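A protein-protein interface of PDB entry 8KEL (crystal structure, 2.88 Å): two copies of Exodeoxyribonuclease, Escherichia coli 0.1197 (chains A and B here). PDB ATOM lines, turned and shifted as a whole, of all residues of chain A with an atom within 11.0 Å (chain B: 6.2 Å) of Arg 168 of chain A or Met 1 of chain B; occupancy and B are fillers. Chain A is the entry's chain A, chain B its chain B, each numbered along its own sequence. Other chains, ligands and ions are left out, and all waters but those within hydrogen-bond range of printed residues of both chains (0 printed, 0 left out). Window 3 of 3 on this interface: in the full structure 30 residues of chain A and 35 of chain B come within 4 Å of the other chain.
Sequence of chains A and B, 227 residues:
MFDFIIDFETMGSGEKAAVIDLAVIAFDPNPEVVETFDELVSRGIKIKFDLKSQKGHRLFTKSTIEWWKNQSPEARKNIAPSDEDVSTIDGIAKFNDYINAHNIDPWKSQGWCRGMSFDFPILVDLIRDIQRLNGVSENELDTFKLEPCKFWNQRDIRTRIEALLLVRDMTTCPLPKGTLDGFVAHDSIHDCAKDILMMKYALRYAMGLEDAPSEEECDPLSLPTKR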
ATOM      1  N   ARG A 158      -1.367  26.503  23.474  1.00  0.00           N
ATOM      2  CA  ARG A 158      -2.091  26.282  22.219  1.00  0.00           C
ATOM      3  C   ARG A 158      -1.990  24.827  21.773  1.00  0.00           C
ATOM      4  O   ARG A 158      -2.952  24.259  21.247  1.00  0.00           O
ATOM      5  CB  ARG A 158      -1.570  27.197  21.107  1.00  0.00           C
ATOM      6  CG  ARG A 158      -1.613  28.670  21.408  1.00  0.00           C
ATOM      7  CD  ARG A 158      -1.194  29.485  20.203  1.00  0.00           C
ATOM      8  NE  ARG A 158      -1.100  30.913  20.498  1.00  0.00           N
ATOM      9  CZ  ARG A 158       0.025  31.593  20.698  1.00  0.00           C
ATOM     10  NH1 ARG A 158       1.216  31.043  20.508  1.00  0.00           N
ATOM     11  NH2 ARG A 158      -0.045  32.869  21.069  1.00  0.00           N
ATOM     12  N   THR A 159      -0.828  24.211  21.953  1.00  0.00           N
ATOM     13  CA  THR A 159      -0.689  22.795  21.613  1.00  0.00           C
ATOM     14  C   THR A 159      -1.575  21.940  22.515  1.00  0.00           C
ATOM     15  O   THR A 159      -2.249  21.017  22.046  1.00  0.00           O
ATOM     16  CB  THR A 159       0.789  22.378  21.718  1.00  0.00           C
ATOM     17  OG1 THR A 159       1.596  23.329  21.027  1.00  0.00           O
ATOM     18  CG2 THR A 159       1.022  21.036  21.065  1.00  0.00           C
ATOM     19  N   ARG A 160      -1.604  22.271  23.811  1.00  0.00           N
ATOM     20  CA  ARG A 160      -2.362  21.526  24.813  1.00  0.00           C
ATOM     21  C   ARG A 160      -3.840  21.491  24.471  1.00  0.00           C
ATOM     22  O   ARG A 160      -4.420  20.420  24.250  1.00  0.00           O
ATOM     23  CB  ARG A 160      -2.151  22.181  26.177  1.00  0.00           C
ATOM     24  CG  ARG A 160      -2.829  21.533  27.338  1.00  0.00           C
ATOM     25  CD  ARG A 160      -2.333  20.161  27.531  1.00  0.00           C
ATOM     26  NE  ARG A 160      -2.786  19.631  28.799  1.00  0.00           N
ATOM     27  CZ  ARG A 160      -2.669  18.364  29.154  1.00  0.00           C
ATOM     28  NH1 ARG A 160      -2.126  17.472  28.342  1.00  0.00           N
ATOM     29  NH2 ARG A 160      -3.101  17.982  30.356  1.00  0.00           N
ATOM     30  N   ILE A 161      -4.459  22.671  24.416  1.00  0.00           N
ATOM     31  CA  ILE A 161      -5.892  22.771  24.155  1.00  0.00           C
ATOM     32  C   ILE A 161      -6.238  22.154  22.810  1.00  0.00           C
ATOM     33  O   ILE A 161      -7.196  21.379  22.698  1.00  0.00           O
ATOM     34  CB  ILE A 161      -6.340  24.234  24.228  1.00  0.00           C
ATOM     35  CG1 ILE A 161      -6.219  24.716  25.667  1.00  0.00           C
ATOM     36  CG2 ILE A 161      -7.730  24.344  23.711  1.00  0.00           C
ATOM     37  CD1 ILE A 161      -6.330  26.198  25.801  1.00  0.00           C
ATOM     38  N   GLU A 162      -5.449  22.476  21.771  1.00  0.00           N
ATOM     39  CA  GLU A 162      -5.695  21.915  20.448  1.00  0.00           C
ATOM     40  C   GLU A 162      -5.577  20.402  20.454  1.00  0.00           C
ATOM     41  O   GLU A 162      -6.279  19.732  19.694  1.00  0.00           O
ATOM     42  CB  GLU A 162      -4.741  22.513  19.414  1.00  0.00           C
ATOM     43  CG  GLU A 162      -4.938  21.961  17.990  1.00  0.00           C
ATOM     44  CD  GLU A 162      -3.961  22.538  16.928  1.00  0.00           C
ATOM     45  OE1 GLU A 162      -3.044  23.330  17.246  1.00  0.00           O
ATOM     46  OE2 GLU A 162      -4.130  22.196  15.737  1.00  0.00           O
ATOM     47  N   ALA A 163      -4.703  19.839  21.287  1.00  0.00           N
ATOM     48  CA  ALA A 163      -4.567  18.387  21.316  1.00  0.00           C
ATOM     49  C   ALA A 163      -5.522  17.724  22.295  1.00  0.00           C
ATOM     50  O   ALA A 163      -5.783  16.518  22.171  1.00  0.00           O
ATOM     51  CB  ALA A 163      -3.134  17.977  21.658  1.00  0.00           C
ATOM     52  N   LEU A 164      -6.036  18.472  23.274  1.00  0.00           N
ATOM     53  CA  LEU A 164      -7.062  17.914  24.142  1.00  0.00           C
ATOM     54  C   LEU A 164      -8.413  17.869  23.448  1.00  0.00           C
ATOM     55  O   LEU A 164      -9.156  16.895  23.611  1.00  0.00           O
ATOM     56  CB  LEU A 164      -7.148  18.704  25.444  1.00  0.00           C
ATOM     57  CG  LEU A 164      -5.985  18.406  26.394  1.00  0.00           C
ATOM     58  CD1 LEU A 164      -5.987  19.346  27.587  1.00  0.00           C
ATOM     59  CD2 LEU A 164      -6.014  16.946  26.848  1.00  0.00           C
ATOM     60  N   LEU A 165      -8.743  18.897  22.660  1.00  0.00           N
ATOM     61  CA  LEU A 165     -10.028  18.946  21.974  1.00  0.00           C
ATOM     62  C   LEU A 165     -10.009  18.228  20.628  1.00  0.00           C
ATOM     63  O   LEU A 165     -11.068  18.036  20.039  1.00  0.00           O
ATOM     64  CB  LEU A 165     -10.484  20.404  21.777  1.00  0.00           C
ATOM     65  CG  LEU A 165     -10.719  21.250  23.052  1.00  0.00           C
ATOM     66  CD1 LEU A 165     -11.034  22.713  22.752  1.00  0.00           C
ATOM     67  CD2 LEU A 165     -11.779  20.679  23.974  1.00  0.00           C
ATOM     68  N   LEU A 166      -8.851  17.805  20.140  1.00  0.00           N
ATOM     69  CA  LEU A 166      -8.732  17.145  18.834  1.00  0.00           C
ATOM     70  C   LEU A 166      -9.385  17.958  17.711  1.00  0.00           C
ATOM     71  O   LEU A 166     -10.089  17.414  16.861  1.00  0.00           O
ATOM     72  CB  LEU A 166      -9.318  15.731  18.852  1.00  0.00           C
ATOM     73  CG  LEU A 166      -8.612  14.562  19.550  1.00  0.00           C
ATOM     74  CD1 LEU A 166      -7.121  14.473  19.181  1.00  0.00           C
ATOM     75  CD2 LEU A 166      -8.829  14.566  21.068  1.00  0.00           C
ATOM     76  N   VAL A 167      -9.148  19.271  17.693  1.00  0.00           N
ATOM     77  CA  VAL A 167      -9.640  20.130  16.615  1.00  0.00           C
ATOM     78  C   VAL A 167      -8.552  21.101  16.173  1.00  0.00           C
ATOM     79  O   VAL A 167      -8.033  21.871  16.984  1.00  0.00           O
ATOM     80  CB  VAL A 167     -10.906  20.896  17.040  1.00  0.00           C
ATOM     81  CG1 VAL A 167     -11.177  22.028  16.078  1.00  0.00           C
ATOM     82  CG2 VAL A 167     -12.084  19.946  17.035  1.00  0.00           C
ATOM     83  N   ARG A 168      -8.248  21.107  14.880  1.00  0.00           N
ATOM     84  CA  ARG A 168      -7.135  21.910  14.391  1.00  0.00           C
ATOM     85  C   ARG A 168      -7.352  23.391  14.687  1.00  0.00           C
ATOM     86  O   ARG A 168      -8.453  23.916  14.536  1.00  0.00           O
ATOM     87  CB  ARG A 168      -6.934  21.712  12.880  1.00  0.00           C
ATOM     88  CG  ARG A 168      -5.682  22.417  12.339  1.00  0.00           C
ATOM     89  CD  ARG A 168      -5.479  22.245  10.832  1.00  0.00           C
ATOM     90  NE  ARG A 168      -4.258  22.921  10.391  1.00  0.00           N
ATOM     91  CZ  ARG A 168      -3.058  22.350  10.340  1.00  0.00           C
ATOM     92  NH1 ARG A 168      -2.886  21.071  10.648  1.00  0.00           N
ATOM     93  NH2 ARG A 168      -2.004  23.075   9.963  1.00  0.00           N
ATOM     94  N   ASP A 169      -6.278  24.059  15.100  1.00  0.00           N
ATOM     95  CA  ASP A 169      -6.245  25.491  15.389  1.00  0.00           C
ATOM     96  C   ASP A 169      -7.280  25.922  16.410  1.00  0.00           C
ATOM     97  O   ASP A 169      -7.603  27.110  16.493  1.00  0.00           O
ATOM     98  CB  ASP A 169      -6.350  26.329  14.106  1.00  0.00           C
ATOM     99  CG  ASP A 169      -4.958  26.656  13.503  1.00  0.00           C
ATOM    100  OD1 ASP A 169      -4.051  27.042  14.285  1.00  0.00           O
ATOM    101  OD2 ASP A 169      -4.740  26.479  12.275  1.00  0.00           O
ATOM    102  N   MET A 170      -7.781  24.999  17.234  1.00  0.00           N
ATOM    103  CA  MET A 170      -8.709  25.361  18.298  1.00  0.00           C
ATOM    104  C   MET A 170      -7.932  25.440  19.607  1.00  0.00           C
ATOM    105  O   MET A 170      -7.624  24.426  20.239  1.00  0.00           O
ATOM    106  CB  MET A 170      -9.883  24.400  18.406  1.00  0.00           C
ATOM    107  CG  MET A 170     -10.916  24.956  19.393  1.00  0.00           C
ATOM    108  SD  MET A 170     -12.506  24.137  19.476  1.00  0.00           S
ATOM    109  CE  MET A 170     -13.242  25.027  20.849  1.00  0.00           C
ATOM    110  N   THR A 171      -7.658  26.666  20.030  1.00  0.00           N
ATOM    111  CA  THR A 171      -6.778  26.922  21.143  1.00  0.00           C
ATOM    112  C   THR A 171      -7.472  27.638  22.296  1.00  0.00           C
ATOM    113  O   THR A 171      -6.798  27.968  23.283  1.00  0.00           O
ATOM    114  CB  THR A 171      -5.577  27.744  20.661  1.00  0.00           C
ATOM    115  OG1 THR A 171      -6.019  29.069  20.350  1.00  0.00           O
ATOM    116  CG2 THR A 171      -5.005  27.130  19.391  1.00  0.00           C
ATOM    117  N   THR A 172      -8.784  27.908  22.201  1.00  0.00           N
ATOM    118  CA  THR A 172      -9.588  28.285  23.362  1.00  0.00           C
ATOM    119  C   THR A 172     -10.703  27.271  23.575  1.00  0.00           C
ATOM    120  O   THR A 172     -11.256  26.711  22.623  1.00  0.00           O
ATOM    121  CB  THR A 172     -10.204  29.681  23.255  1.00  0.00           C
ATOM    122  OG1 THR A 172     -11.194  29.705  22.227  1.00  0.00           O
ATOM    123  CG2 THR A 172      -9.141  30.715  22.972  1.00  0.00           C
ATOM    124  N   MET B   1      -1.905  20.901   1.518  1.00  0.00           N
ATOM    125  CA  MET B   1      -1.192  21.587   2.600  1.00  0.00           C
ATOM    126  C   MET B   1      -0.459  20.657   3.570  1.00  0.00           C
ATOM    127  O   MET B   1      -1.058  19.721   4.113  1.00  0.00           O
ATOM    128  CB  MET B   1      -2.138  22.426   3.451  1.00  0.00           C
ATOM    129  CG  MET B   1      -1.370  23.175   4.534  1.00  0.00           C
ATOM    130  SD  MET B   1      -2.311  23.769   5.948  1.00  0.00           S
ATOM    131  CE  MET B   1      -2.548  22.229   6.840  1.00  0.00           C
ATOM    132  N   PHE B   2       0.811  20.971   3.844  1.00  0.00           N
ATOM    133  CA  PHE B   2       1.631  20.221   4.783  1.00  0.00           C
ATOM    134  C   PHE B   2       2.010  21.049   6.004  1.00  0.00           C
ATOM    135  O   PHE B   2       2.139  22.274   5.938  1.00  0.00           O
ATOM    136  CB  PHE B   2       2.931  19.728   4.139  1.00  0.00           C
ATOM    137  CG  PHE B   2       2.757  18.557   3.242  1.00  0.00           C
ATOM    138  CD1 PHE B   2       1.518  17.991   3.058  1.00  0.00           C
ATOM    139  CD2 PHE B   2       3.853  17.951   2.671  1.00  0.00           C
ATOM    140  CE1 PHE B   2       1.363  16.892   2.251  1.00  0.00           C
ATOM    141  CE2 PHE B   2       3.707  16.835   1.868  1.00  0.00           C
ATOM    142  CZ  PHE B   2       2.460  16.308   1.658  1.00  0.00           C
ATOM    143  N   ASP B   3       2.189  20.358   7.123  1.00  0.00           N
ATOM    144  CA  ASP B   3       2.960  20.862   8.246  1.00  0.00           C
ATOM    145  C   ASP B   3       4.428  20.436   8.101  1.00  0.00           C
ATOM    146  O   ASP B   3       4.779  19.562   7.302  1.00  0.00           O
ATOM    147  CB  ASP B   3       2.389  20.355   9.567  1.00  0.00           C
ATOM    148  CG  ASP B   3       1.095  21.036   9.946  1.00  0.00           C
ATOM    149  OD1 ASP B   3       0.901  22.208   9.556  1.00  0.00           O
ATOM    150  OD2 ASP B   3       0.275  20.413  10.661  1.00  0.00           O
ATOM    151  N   PHE B  27       5.665  17.016   6.452  1.00  0.00           N
ATOM    152  CA  PHE B  27       4.837  15.832   6.551  1.00  0.00           C
ATOM    153  C   PHE B  27       3.369  16.197   6.367  1.00  0.00           C
ATOM    154  O   PHE B  27       2.976  17.363   6.474  1.00  0.00           O
ATOM    155  CB  PHE B  27       5.063  15.161   7.905  1.00  0.00           C
ATOM    156  CG  PHE B  27       4.716  16.037   9.091  1.00  0.00           C
ATOM    157  CD1 PHE B  27       5.602  16.989   9.545  1.00  0.00           C
ATOM    158  CD2 PHE B  27       3.523  15.876   9.768  1.00  0.00           C
ATOM    159  CE1 PHE B  27       5.304  17.779  10.631  1.00  0.00           C
ATOM    160  CE2 PHE B  27       3.222  16.659  10.857  1.00  0.00           C
ATOM    161  CZ  PHE B  27       4.115  17.608  11.295  1.00  0.00           C
ATOM    162  N   ASP B  28       2.558  15.172   6.096  1.00  0.00           N
ATOM    163  CA  ASP B  28       1.139  15.338   5.819  1.00  0.00           C
ATOM    164  C   ASP B  28       0.344  15.135   7.102  1.00  0.00           C
ATOM    165  O   ASP B  28       0.268  14.001   7.597  1.00  0.00           O
ATOM    166  CB  ASP B  28       0.708  14.338   4.744  1.00  0.00           C
ATOM    167  CG  ASP B  28      -0.752  14.485   4.308  1.00  0.00           C
ATOM    168  OD1 ASP B  28      -1.519  15.268   4.936  1.00  0.00           O
ATOM    169  OD2 ASP B  28      -1.122  13.811   3.307  1.00  0.00           O
ATOM    170  N   PRO B  29      -0.292  16.176   7.652  1.00  0.00           N
ATOM    171  CA  PRO B  29      -0.879  16.063   8.999  1.00  0.00           C
ATOM    172  C   PRO B  29      -2.156  15.243   9.087  1.00  0.00           C
ATOM    173  O   PRO B  29      -2.661  15.069  10.198  1.00  0.00           O
ATOM    174  CB  PRO B  29      -1.141  17.519   9.380  1.00  0.00           C
ATOM    175  CG  PRO B  29      -1.293  18.214   8.093  1.00  0.00           C
ATOM    176  CD  PRO B  29      -0.397  17.544   7.117  1.00  0.00           C
ATOM    177  N   HIS B 102       7.592  22.470  -0.656  1.00  0.00           N
ATOM    178  CA  HIS B 102       6.875  21.350  -0.058  1.00  0.00           C
ATOM    179  C   HIS B 102       5.536  21.775   0.482  1.00  0.00           C
ATOM    180  O   HIS B 102       5.138  21.393   1.581  1.00  0.00           O
ATOM    181  CB  HIS B 102       7.701  20.678   1.014  1.00  0.00           C
ATOM    182  CG  HIS B 102       8.792  19.824   0.457  1.00  0.00           C
ATOM    183  ND1 HIS B 102      10.052  20.307   0.181  1.00  0.00           N
ATOM    184  CD2 HIS B 102       8.794  18.526   0.075  1.00  0.00           C
ATOM    185  CE1 HIS B 102      10.790  19.336  -0.324  1.00  0.00           C
ATOM    186  NE2 HIS B 102      10.050  18.245  -0.397  1.00  0.00           N
ATOM    187  N   ASN B 103       4.809  22.545  -0.329  1.00  0.00           N
ATOM    188  CA  ASN B 103       3.389  22.803  -0.128  1.00  0.00           C
ATOM    189  C   ASN B 103       3.114  23.242   1.312  1.00  0.00           C
ATOM    190  O   ASN B 103       2.233  22.722   2.001  1.00  0.00           O
ATOM    191  CB  ASN B 103       2.556  21.578  -0.525  1.00  0.00           C
ATOM    192  N   ILE B 104       3.913  24.196   1.773  1.00  0.00           N
ATOM    193  CA  ILE B 104       3.773  24.781   3.100  1.00  0.00           C
ATOM    194  C   ILE B 104       3.013  26.089   2.948  1.00  0.00           C
ATOM    195  O   ILE B 104       3.413  26.958   2.162  1.00  0.00           O
ATOM    196  CB  ILE B 104       5.144  24.995   3.771  1.00  0.00           C
ATOM    197  CG1 ILE B 104       5.881  23.666   3.937  1.00  0.00           C
ATOM    198  CG2 ILE B 104       4.993  25.633   5.138  1.00  0.00           C
ATOM    199  CD1 ILE B 104       5.153  22.670   4.838  1.00  0.00           C
ATOM    200  N   ASP B 105       1.910  26.215   3.685  1.00  0.00           N
ATOM    201  CA  ASP B 105       1.015  27.367   3.602  1.00  0.00           C
ATOM    202  C   ASP B 105       1.456  28.431   4.603  1.00  0.00           C
ATOM    203  O   ASP B 105       1.585  28.126   5.797  1.00  0.00           O
ATOM    204  CB  ASP B 105      -0.425  26.919   3.873  1.00  0.00           C
ATOM    205  CG  ASP B 105      -1.464  28.010   3.642  1.00  0.00           C
ATOM    206  OD1 ASP B 105      -1.113  29.190   3.465  1.00  0.00           O
ATOM    207  OD2 ASP B 105      -2.663  27.664   3.598  1.00  0.00           O
ATOM    208  N   LYS B 108      -1.865  28.771   7.075  1.00  0.00           N
ATOM    209  CA  LYS B 108      -2.532  27.632   7.686  1.00  0.00           C
ATOM    210  C   LYS B 108      -1.562  26.606   8.258  1.00  0.00           C
ATOM    211  O   LYS B 108      -1.887  25.949   9.255  1.00  0.00           O
ATOM    212  CB  LYS B 108      -3.467  26.975   6.662  1.00  0.00           C
ATOM    213  CG  LYS B 108      -4.700  27.830   6.314  1.00  0.00           C
ATOM    214  CD  LYS B 108      -5.514  27.319   5.099  1.00  0.00           C
ATOM    215  CE  LYS B 108      -6.368  26.083   5.401  1.00  0.00           C
ATOM    216  NZ  LYS B 108      -7.263  25.679   4.252  1.00  0.00           N
ATOM    217  N   SER B 109      -0.374  26.476   7.671  1.00  0.00           N
ATOM    218  CA  SER B 109       0.571  25.443   8.076  1.00  0.00           C
ATOM    219  C   SER B 109       1.138  25.674   9.472  1.00  0.00           C
ATOM    220  O   SER B 109       1.316  26.811   9.927  1.00  0.00           O
ATOM    221  CB  SER B 109       1.723  25.356   7.092  1.00  0.00           C
ATOM    222  OG  SER B 109       1.273  24.838   5.872  1.00  0.00           O
ATOM    223  N   GLN B 110       1.464  24.564  10.128  1.00  0.00           N
ATOM    224  CA  GLN B 110       2.018  24.546  11.466  1.00  0.00           C
ATOM    225  C   GLN B 110       3.450  24.032  11.432  1.00  0.00           C
ATOM    226  O   GLN B 110       3.787  23.140  10.641  1.00  0.00           O
ATOM    227  CB  GLN B 110       1.155  23.681  12.385  1.00  0.00           C
ATOM    228  CG  GLN B 110      -0.180  24.346  12.709  1.00  0.00           C
ATOM    229  CD  GLN B 110      -1.133  23.465  13.496  1.00  0.00           C
ATOM    230  OE1 GLN B 110      -0.880  22.272  13.718  1.00  0.00           O
ATOM    231  NE2 GLN B 110      -2.244  24.054  13.922  1.00  0.00           N
ATOM    232  N   ASN B 153       1.007  29.440  14.994  1.00  0.00           N
ATOM    233  CA  ASN B 153       0.951  28.089  14.447  1.00  0.00           C
ATOM    234  C   ASN B 153       2.180  27.261  14.781  1.00  0.00           C
ATOM    235  O   ASN B 153       2.306  26.136  14.285  1.00  0.00           O
ATOM    236  CB  ASN B 153       0.786  28.106  12.936  1.00  0.00           C
ATOM    237  CG  ASN B 153      -0.514  28.684  12.509  1.00  0.00           C
ATOM    238  OD1 ASN B 153      -0.543  29.690  11.806  1.00  0.00           O
ATOM    239  ND2 ASN B 153      -1.608  28.067  12.938  1.00  0.00           N
ATOM    240  N   ARG B 155       4.251  24.854  17.230  1.00  0.00           N
ATOM    241  CA  ARG B 155       3.739  23.768  18.047  1.00  0.00           C
ATOM    242  C   ARG B 155       4.889  22.995  18.684  1.00  0.00           C
ATOM    243  O   ARG B 155       5.984  22.892  18.120  1.00  0.00           O
ATOM    244  CB  ARG B 155       2.861  22.820  17.227  1.00  0.00           C
ATOM    245  CG  ARG B 155       1.549  23.416  16.733  1.00  0.00           C
ATOM    246  CD  ARG B 155       0.564  23.674  17.874  1.00  0.00           C
ATOM    247  NE  ARG B 155      -0.744  24.121  17.397  1.00  0.00           N
ATOM    248  CZ  ARG B 155      -1.092  25.387  17.204  1.00  0.00           C
ATOM    249  NH1 ARG B 155      -0.241  26.382  17.412  1.00  0.00           N
ATOM    250  NH2 ARG B 155      -2.322  25.661  16.783  1.00  0.00           N
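Among the printed residues, pairs that only touch across the chains: Thr 159 of chain A with Arg 155 of chain B (3.3 Å), Arg 168 of chain A with Met 1 of chain B (3.3 Å), Arg 168 of chain A with Ser 109 of chain B (3.97 Å), Arg 168 of chain A with Gln 110 of chain B (3.5 Å) and Asp 169 of chain A with Gln 110 of chain B (3.5 Å).
The guanidinium group of Arg 168 of chain A is in salt-bridge range of the side-chain carboxylate of Asp 3 of chain B (3.1 Å). ND2 of Asn 153 of chain B lies within hydrogen-bond range of OD1 of Asp 169 of chain A, at 3.0 Å. The guanidinium group (NE) of Arg 155 of chain B is in salt-bridge range of the side-chain carboxylate (OE1) of Glu 162 of chain A (2.4 Å). NH2 of Arg 155 of chain B lies within salt-bridge range of OD1 of Asp 169 of chain A (3.3 Å). NH2 of Arg 168 of chain A lies within hydrogen-bond range of O of Lys 108 of chain B (3.0 Å). The side-chain carboxylate (OE2) of Glu 162 of chain A is in hydrogen-bond range of the side-chain amide nitrogen (NE2) of Gln 110 of chain B, 3.2 Å away.
Of the printed residues of chain B, Thr 159 of chain A touches Arg 155 (3.3 Å). Printed residues of chain B within 4 Å of Glu 162 of chain A: Gln 110 (3.2 Å) and Arg 155 (2.4 Å). Val 167 of chain A touches none of the printed residues of chain B. Of chain B, only Met 1, Asp 3, Lys 108, Ser 109 and Gln 110 come within 4 Å of Arg 168 of chain A. Of the printed residues of chain B, Asp 169 of chain A touches Gln 110 (3.5 Å), Asn 153 (3.0 Å) and Arg 155 (3.3 Å). Thr 171 of chain A touches none of the printed residues of chain B. Met 1 of chain B touches one residue of chain A. Phe 2 of chain B touches none of the printed residues of chain A. Of chain A, only Arg 168 comes within 4 Å of Asp 3 of chain B. Asp 28 of chain B touches none of the printed residues of chain A. No residue of chain A comes within 4 Å of Asn 103 of chain B. No residue of chain A comes within 4 Å of Asp 105 of chain B. Lys 108 of chain B touches just one residue of chain A: Arg 168 (3.0 Å). Of chain A, only Arg 168 comes within 4 Å of Ser 109 of chain B. Gln 110 of chain B touches just these residues of chain A: Glu 162 (3.2 Å), Arg 168 (3.5 Å) and Asp 169 (3.5 Å). Of the printed residues of chain A, Asn 153 of chain B touches Asp 169 (3.0 Å). Printed residues of chain A within 4 Å of Arg 155 of chain B: Thr 159 (3.3 Å), Glu 162 (2.4 Å) and Asp 169 (3.3 Å).
O of Phe 2 of chain B is in hydrogen-bond range of OG of Ser 109 of chain B (2.7 Å). The side-chain carboxylate (OD1) of Asp 3 of chain B lies within hydrogen-bond range of the backbone NH (N) of Gln 110 of chain B (2.5 Å). The backbone NH of Phe 27 of chain B is in hydrogen-bond range of the backbone carbonyl oxygen of Asp 3 of chain B, at 2.8 Å. The backbone NH (N) of Glu 162 of chain A lies close to the backbone carbonyl oxygen (O) of Met 170 of chain A (3.3 Å). The backbone NH (N) of Asp 105 of chain B is in hydrogen-bond range of the side-chain hydroxyl (OG) of Ser 109 of chain B. The side-chain sulfur (SD) of Met 1 of chain B sits close to the side-chain hydroxyl (OG) of Ser 109 of chain B (3.7 Å).
No position is printed for both chains.
Printed residues of chain B that touch a printed residue of chain A: Met 1, Asp 3, Lys 108, Ser 109, Gln 110, Asn 153 and Arg 155. Hydrophobic or aromatic side chains of chain B that line the printed part of chain A: Met 1. Along chain B the printed residues that touch a printed residue of chain A span positions 1 to 155. Of the 15 printed residues of chain A, 4 touch a printed residue of chain B. Printed residues of chain A that touch a printed residue of chain B: Thr 159, Glu 162, Arg 168 and Asp 169. Among the printed residues, 11 pairs touch across the chains. Among the printed residues, Asp or Glu carboxylates within 4 Å of a Lys or Arg side-chain nitrogen of the other chain: Glu 162 of chain A with Arg 155 of chain B, Arg 168 of chain A with Asp 3 of chain B and Asp 169 of chain A with Arg 155 of chain B.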
